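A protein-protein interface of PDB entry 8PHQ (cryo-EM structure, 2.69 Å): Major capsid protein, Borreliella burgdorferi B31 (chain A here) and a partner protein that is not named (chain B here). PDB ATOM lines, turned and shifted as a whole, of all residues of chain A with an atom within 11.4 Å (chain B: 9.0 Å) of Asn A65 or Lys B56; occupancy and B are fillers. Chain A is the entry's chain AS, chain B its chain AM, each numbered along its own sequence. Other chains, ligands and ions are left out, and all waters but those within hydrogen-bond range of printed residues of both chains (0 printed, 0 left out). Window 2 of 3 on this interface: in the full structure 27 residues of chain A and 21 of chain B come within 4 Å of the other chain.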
ATOM      1  N   THR A  58      -7.510   5.967   8.173  1.00  0.00           N
ATOM      2  CA  THR A  58      -8.713   5.343   8.706  1.00  0.00           C
ATOM      3  C   THR A  58      -8.487   3.846   8.875  1.00  0.00           C
ATOM      4  O   THR A  58      -8.031   3.173   7.946  1.00  0.00           O
ATOM      5  CB  THR A  58      -9.907   5.596   7.786  1.00  0.00           C
ATOM      6  OG1 THR A  58     -10.207   6.996   7.765  1.00  0.00           O
ATOM      7  CG2 THR A  58     -11.128   4.832   8.267  1.00  0.00           C
ATOM      8  N   THR A  59      -8.808   3.333  10.060  1.00  0.00           N
ATOM      9  CA  THR A  59      -8.703   1.906  10.328  1.00  0.00           C
ATOM     10  C   THR A  59      -9.862   1.171   9.671  1.00  0.00           C
ATOM     11  O   THR A  59     -11.029   1.503   9.901  1.00  0.00           O
ATOM     12  CB  THR A  59      -8.699   1.642  11.832  1.00  0.00           C
ATOM     13  OG1 THR A  59      -7.574   2.294  12.432  1.00  0.00           O
ATOM     14  CG2 THR A  59      -8.617   0.152  12.111  1.00  0.00           C
ATOM     15  N   ILE A  60      -9.542   0.170   8.854  1.00  0.00           N
ATOM     16  CA  ILE A  60     -10.559  -0.610   8.145  1.00  0.00           C
ATOM     17  C   ILE A  60     -10.911  -1.793   9.041  1.00  0.00           C
ATOM     18  O   ILE A  60     -10.287  -2.853   8.993  1.00  0.00           O
ATOM     19  CB  ILE A  60     -10.087  -1.043   6.760  1.00  0.00           C
ATOM     20  CG1 ILE A  60      -9.695   0.182   5.940  1.00  0.00           C
ATOM     21  CG2 ILE A  60     -11.177  -1.820   6.048  1.00  0.00           C
ATOM     22  CD1 ILE A  60     -10.819   1.182   5.788  1.00  0.00           C
ATOM     23  N   ALA A  61     -11.928  -1.599   9.876  1.00  0.00           N
ATOM     24  CA  ALA A  61     -12.464  -2.652  10.725  1.00  0.00           C
ATOM     25  C   ALA A  61     -13.981  -2.574  10.686  1.00  0.00           C
ATOM     26  O   ALA A  61     -14.548  -1.488  10.837  1.00  0.00           O
ATOM     27  CB  ALA A  61     -11.957  -2.519  12.164  1.00  0.00           C
ATOM     28  N   ASN A  62     -14.625  -3.716  10.485  1.00  0.00           N
ATOM     29  CA  ASN A  62     -16.092  -3.810  10.380  1.00  0.00           C
ATOM     30  C   ASN A  62     -16.528  -2.934   9.200  1.00  0.00           C
ATOM     31  O   ASN A  62     -15.849  -2.917   8.163  1.00  0.00           O
ATOM     32  CB  ASN A  62     -16.734  -3.467  11.709  1.00  0.00           C
ATOM     33  CG  ASN A  62     -16.466  -4.509  12.772  1.00  0.00           C
ATOM     34  OD1 ASN A  62     -15.814  -5.521  12.515  1.00  0.00           O
ATOM     35  ND2 ASN A  62     -16.965  -4.268  13.976  1.00  0.00           N
ATOM     36  N   GLU A  63     -17.633  -2.204   9.319  1.00  0.00           N
ATOM     37  CA  GLU A  63     -18.157  -1.380   8.240  1.00  0.00           C
ATOM     38  C   GLU A  63     -17.883   0.089   8.523  1.00  0.00           C
ATOM     39  O   GLU A  63     -18.056   0.557   9.652  1.00  0.00           O
ATOM     40  CB  GLU A  63     -19.661  -1.597   8.064  1.00  0.00           C
ATOM     41  CG  GLU A  63     -20.053  -3.026   7.756  1.00  0.00           C
ATOM     42  CD  GLU A  63     -21.552  -3.232   7.785  1.00  0.00           C
ATOM     43  OE1 GLU A  63     -22.265  -2.512   7.055  1.00  0.00           O
ATOM     44  OE2 GLU A  63     -22.018  -4.110   8.540  1.00  0.00           O
ATOM     45  N   VAL A  64     -17.458   0.812   7.492  1.00  0.00           N
ATOM     46  CA  VAL A  64     -17.213   2.244   7.605  1.00  0.00           C
ATOM     47  C   VAL A  64     -17.315   2.853   6.214  1.00  0.00           C
ATOM     48  O   VAL A  64     -16.842   2.278   5.230  1.00  0.00           O
ATOM     49  CB  VAL A  64     -15.847   2.530   8.277  1.00  0.00           C
ATOM     50  CG1 VAL A  64     -14.697   2.018   7.425  1.00  0.00           C
ATOM     51  CG2 VAL A  64     -15.691   4.014   8.556  1.00  0.00           C
ATOM     52  N   ASN A  65     -17.971   4.013   6.136  1.00  0.00           N
ATOM     53  CA  ASN A  65     -18.133   4.737   4.885  1.00  0.00           C
ATOM     54  C   ASN A  65     -17.326   6.021   4.817  1.00  0.00           C
ATOM     55  O   ASN A  65     -17.098   6.528   3.717  1.00  0.00           O
ATOM     56  CB  ASN A  65     -19.611   5.088   4.652  1.00  0.00           C
ATOM     57  CG  ASN A  65     -20.478   3.869   4.448  1.00  0.00           C
ATOM     58  OD1 ASN A  65     -20.289   3.109   3.501  1.00  0.00           O
ATOM     59  ND2 ASN A  65     -21.448   3.681   5.333  1.00  0.00           N
ATOM     60  N   THR A  66     -16.894   6.553   5.955  1.00  0.00           N
ATOM     61  CA  THR A  66     -16.277   7.871   6.029  1.00  0.00           C
ATOM     62  C   THR A  66     -14.769   7.684   6.179  1.00  0.00           C
ATOM     63  O   THR A  66     -14.289   7.301   7.250  1.00  0.00           O
ATOM     64  CB  THR A  66     -16.863   8.659   7.196  1.00  0.00           C
ATOM     65  OG1 THR A  66     -18.280   8.763   7.028  1.00  0.00           O
ATOM     66  CG2 THR A  66     -16.299  10.055   7.230  1.00  0.00           C
ATOM     67  N   ILE A  67     -14.027   7.958   5.107  1.00  0.00           N
ATOM     68  CA  ILE A  67     -12.595   7.697   5.047  1.00  0.00           C
ATOM     69  C   ILE A  67     -11.850   9.015   4.897  1.00  0.00           C
ATOM     70  O   ILE A  67     -12.322   9.946   4.238  1.00  0.00           O
ATOM     71  CB  ILE A  67     -12.246   6.739   3.887  1.00  0.00           C
ATOM     72  CG1 ILE A  67     -13.215   5.556   3.854  1.00  0.00           C
ATOM     73  CG2 ILE A  67     -10.816   6.244   4.009  1.00  0.00           C
ATOM     74  CD1 ILE A  67     -13.113   4.648   5.052  1.00  0.00           C
ATOM     75  N   SER A  68     -10.673   9.089   5.517  1.00  0.00           N
ATOM     76  CA  SER A  68      -9.838  10.278   5.410  1.00  0.00           C
ATOM     77  C   SER A  68      -9.363  10.472   3.975  1.00  0.00           C
ATOM     78  O   SER A  68      -9.185   9.514   3.219  1.00  0.00           O
ATOM     79  CB  SER A  68      -8.637  10.173   6.349  1.00  0.00           C
ATOM     80  OG  SER A  68      -9.042  10.254   7.703  1.00  0.00           O
ATOM     81  N   THR A  69      -9.150  11.729   3.603  1.00  0.00           N
ATOM     82  CA  THR A  69      -8.882  12.098   2.223  1.00  0.00           C
ATOM     83  C   THR A  69      -7.460  12.615   2.047  1.00  0.00           C
ATOM     84  O   THR A  69      -6.812  13.072   2.991  1.00  0.00           O
ATOM     85  CB  THR A  69      -9.875  13.160   1.738  1.00  0.00           C
ATOM     86  OG1 THR A  69      -9.753  14.334   2.547  1.00  0.00           O
ATOM     87  CG2 THR A  69     -11.297  12.638   1.819  1.00  0.00           C
ATOM     88  N   CYS B  52     -12.308  14.339   5.991  1.00  0.00           N
ATOM     89  CA  CYS B  52     -12.708  12.938   6.056  1.00  0.00           C
ATOM     90  C   CYS B  52     -14.119  12.848   5.489  1.00  0.00           C
ATOM     91  O   CYS B  52     -15.069  13.339   6.104  1.00  0.00           O
ATOM     92  CB  CYS B  52     -12.639  12.420   7.493  1.00  0.00           C
ATOM     93  SG  CYS B  52     -13.000  10.670   7.700  1.00  0.00           S
ATOM     94  N   THR B  53     -14.254  12.223   4.322  1.00  0.00           N
ATOM     95  CA  THR B  53     -15.463  12.305   3.517  1.00  0.00           C
ATOM     96  C   THR B  53     -16.088  10.928   3.343  1.00  0.00           C
ATOM     97  O   THR B  53     -15.380   9.928   3.190  1.00  0.00           O
ATOM     98  CB  THR B  53     -15.151  12.917   2.142  1.00  0.00           C
ATOM     99  OG1 THR B  53     -14.563  14.211   2.319  1.00  0.00           O
ATOM    100  CG2 THR B  53     -16.410  13.060   1.305  1.00  0.00           C
ATOM    101  N   SER B  54     -17.417  10.884   3.363  1.00  0.00           N
ATOM    102  CA  SER B  54     -18.174   9.663   3.147  1.00  0.00           C
ATOM    103  C   SER B  54     -18.651   9.580   1.702  1.00  0.00           C
ATOM    104  O   SER B  54     -18.965  10.592   1.074  1.00  0.00           O
ATOM    105  CB  SER B  54     -19.376   9.591   4.088  1.00  0.00           C
ATOM    106  OG  SER B  54     -20.169   8.452   3.816  1.00  0.00           O
ATOM    107  N   SER B  55     -18.702   8.355   1.180  1.00  0.00           N
ATOM    108  CA  SER B  55     -19.188   8.136  -0.175  1.00  0.00           C
ATOM    109  C   SER B  55     -20.694   8.311  -0.295  1.00  0.00           C
ATOM    110  O   SER B  55     -21.209   8.330  -1.418  1.00  0.00           O
ATOM    111  CB  SER B  55     -18.796   6.740  -0.658  1.00  0.00           C
ATOM    112  OG  SER B  55     -19.241   5.744   0.245  1.00  0.00           O
ATOM    113  N   LYS B  56     -21.409   8.432   0.824  1.00  0.00           N
ATOM    114  CA  LYS B  56     -22.858   8.578   0.825  1.00  0.00           C
ATOM    115  C   LYS B  56     -23.298  10.003   1.140  1.00  0.00           C
ATOM    116  O   LYS B  56     -24.465  10.228   1.473  1.00  0.00           O
ATOM    117  CB  LYS B  56     -23.484   7.597   1.816  1.00  0.00           C
ATOM    118  CG  LYS B  56     -23.012   6.164   1.643  1.00  0.00           C
ATOM    119  CD  LYS B  56     -23.335   5.642   0.254  1.00  0.00           C
ATOM    120  CE  LYS B  56     -22.543   4.387  -0.059  1.00  0.00           C
ATOM    121  NZ  LYS B  56     -22.612   3.407   1.056  1.00  0.00           N
ATOM    122  N   ASP B  57     -22.388  10.968   1.049  1.00  0.00           N
ATOM    123  CA  ASP B  57     -22.743  12.357   1.297  1.00  0.00           C
ATOM    124  C   ASP B  57     -23.580  12.912   0.152  1.00  0.00           C
ATOM    125  O   ASP B  57     -23.390  12.548  -1.012  1.00  0.00           O
ATOM    126  CB  ASP B  57     -21.485  13.204   1.480  1.00  0.00           C
ATOM    127  CG  ASP B  57     -20.872  13.050   2.855  1.00  0.00           C
ATOM    128  OD1 ASP B  57     -21.592  13.248   3.856  1.00  0.00           O
ATOM    129  OD2 ASP B  57     -19.667  12.735   2.936  1.00  0.00           O
ATOM    130  N   LYS B  58     -24.515  13.797   0.487  1.00  0.00           N
ATOM    131  CA  LYS B  58     -25.327  14.479  -0.511  1.00  0.00           C
ATOM    132  C   LYS B  58     -24.700  15.825  -0.845  1.00  0.00           C
ATOM    133  O   LYS B  58     -24.414  16.625   0.051  1.00  0.00           O
ATOM    134  CB  LYS B  58     -26.760  14.667  -0.014  1.00  0.00           C
ATOM    135  CG  LYS B  58     -27.683  15.290  -1.045  1.00  0.00           C
ATOM    136  CD  LYS B  58     -29.097  15.433  -0.518  1.00  0.00           C
ATOM    137  CE  LYS B  58     -30.036  15.926  -1.603  1.00  0.00           C
ATOM    138  NZ  LYS B  58     -31.430  16.076  -1.111  1.00  0.00           N
ATOM    139  N   ILE B  59     -24.489  16.070  -2.135  1.00  0.00           N
ATOM    140  CA  ILE B  59     -23.797  17.256  -2.623  1.00  0.00           C
ATOM    141  C   ILE B  59     -24.707  17.975  -3.608  1.00  0.00           C
ATOM    142  O   ILE B  59     -25.248  17.349  -4.526  1.00  0.00           O
ATOM    143  CB  ILE B  59     -22.457  16.887  -3.285  1.00  0.00           C
ATOM    144  CG1 ILE B  59     -21.583  16.090  -2.316  1.00  0.00           C
ATOM    145  CG2 ILE B  59     -21.740  18.127  -3.763  1.00  0.00           C
ATOM    146  CD1 ILE B  59     -20.299  15.581  -2.927  1.00  0.00           C
ATOM    147  N   ILE B 111     -23.128  21.489   0.932  1.00  0.00           N
ATOM    148  CA  ILE B 111     -23.513  20.325   1.721  1.00  0.00           C
ATOM    149  C   ILE B 111     -24.642  20.758   2.651  1.00  0.00           C
ATOM    150  O   ILE B 111     -24.449  21.679   3.458  1.00  0.00           O
ATOM    151  CB  ILE B 111     -22.326  19.759   2.515  1.00  0.00           C
ATOM    152  CG1 ILE B 111     -21.178  19.418   1.566  1.00  0.00           C
ATOM    153  CG2 ILE B 111     -22.747  18.533   3.301  1.00  0.00           C
ATOM    154  CD1 ILE B 111     -19.956  18.871   2.255  1.00  0.00           C
ATOM    155  N   THR B 114     -28.576  19.170   6.920  1.00  0.00           N
ATOM    156  CA  THR B 114     -29.060  17.857   7.326  1.00  0.00           C
ATOM    157  C   THR B 114     -28.040  16.754   7.080  1.00  0.00           C
ATOM    158  O   THR B 114     -28.362  15.576   7.265  1.00  0.00           O
ATOM    159  CB  THR B 114     -30.363  17.524   6.595  1.00  0.00           C
ATOM    160  OG1 THR B 114     -30.156  17.615   5.181  1.00  0.00           O
ATOM    161  CG2 THR B 114     -31.463  18.486   7.004  1.00  0.00           C
ATOM    162  N   ASN B 115     -26.827  17.111   6.666  1.00  0.00           N
ATOM    163  CA  ASN B 115     -25.755  16.157   6.413  1.00  0.00           C
ATOM    164  C   ASN B 115     -24.517  16.644   7.148  1.00  0.00           C
ATOM    165  O   ASN B 115     -24.069  17.772   6.926  1.00  0.00           O
ATOM    166  CB  ASN B 115     -25.489  16.024   4.911  1.00  0.00           C
ATOM    167  CG  ASN B 115     -24.532  14.898   4.583  1.00  0.00           C
ATOM    168  OD1 ASN B 115     -24.028  14.212   5.469  1.00  0.00           O
ATOM    169  ND2 ASN B 115     -24.281  14.700   3.296  1.00  0.00           N
ATOM    170  N   ASN B 116     -23.970  15.803   8.019  1.00  0.00           N
ATOM    171  CA  ASN B 116     -22.832  16.214   8.828  1.00  0.00           C
ATOM    172  C   ASN B 116     -21.588  16.385   7.962  1.00  0.00           C
ATOM    173  O   ASN B 116     -21.432  15.746   6.920  1.00  0.00           O
ATOM    174  CB  ASN B 116     -22.570  15.206   9.945  1.00  0.00           C
ATOM    175  CG  ASN B 116     -22.029  13.893   9.428  1.00  0.00           C
ATOM    176  OD1 ASN B 116     -22.647  13.244   8.589  1.00  0.00           O
ATOM    177  ND2 ASN B 116     -20.870  13.492   9.934  1.00  0.00           N
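OD1 of Asn A65 lies within hydrogen-bond range of NZ of Lys B56, at 3.4 Å. The backbone carbonyl oxygen of Thr A66 lies close to the side-chain sulfur of Cys B52 (3.6 Å). The backbone carbonyl oxygen (O) of Ile A67 lies close to the side-chain sulfur (SG) of Cys B52 (3.6 Å). The backbone carbonyl oxygen (O) of Ile A67 sits at hydrogen-bond distance from the backbone NH (N) of Thr B53. SG of Cys B52 is in hydrogen-bond range of N of Ser A68.
OG1 of Thr A58 sits at hydrogen-bond distance from N of Ser A68 (3.1 Å). The side-chain hydroxyl of Ser B54 sits close to the backbone NH of Lys B56, 3.2 Å away. The side-chain carboxylate (OD2) of Asp B57 lies within hydrogen-bond range of the backbone NH (N) of Ser B54, at 2.9 Å.
Asn A65 touches Thr B53 (O to O, 3.8 Å). Asn A65 touches Ser B54. Asn A65 touches Ser B55 (O to N, 3.5 Å). Thr B53 touches Thr A66. OG1 of Thr A66 touches CB of Ser B54 (3.2 Å). Thr B53 touches Thr A69.
Of chain B, only Thr B53 (3.8 Å), Ser B54 (3.4 Å), Ser B55 (3.5 Å) and Lys B56 (3.4 Å) come within 4 Å of Asn A65. No residue of chain B comes within 4 Å of Val A64. Of chain B, only Cys B52, Thr B53 and Ser B54 come within 4 Å of Thr A66. Printed residues of chain A within 4 Å of Ser B54: Asn A65 and Thr A66. Of the printed residues of chain A, Ser B55 touches Asn A65. No residue of chain A comes within 4 Å of Asp B57. Printed residues of chain A within 4 Å of Thr B53: Asn A65, Thr A66, Ile A67 and Thr A69. Printed residues of chain B within 4 Å of Ile A67: Cys B52 (3.5 Å) and Thr B53 (3.0 Å). The nearest residue of chain B that does not touch Asn A65 is Asp B57 (6.8 Å).
Of the 12 printed residues of chain B, 5 touch a printed residue of chain A. Of the 12 printed residues of chain A, 5 touch a printed residue of chain B. Among the printed residues, 11 pairs touch across the chains.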
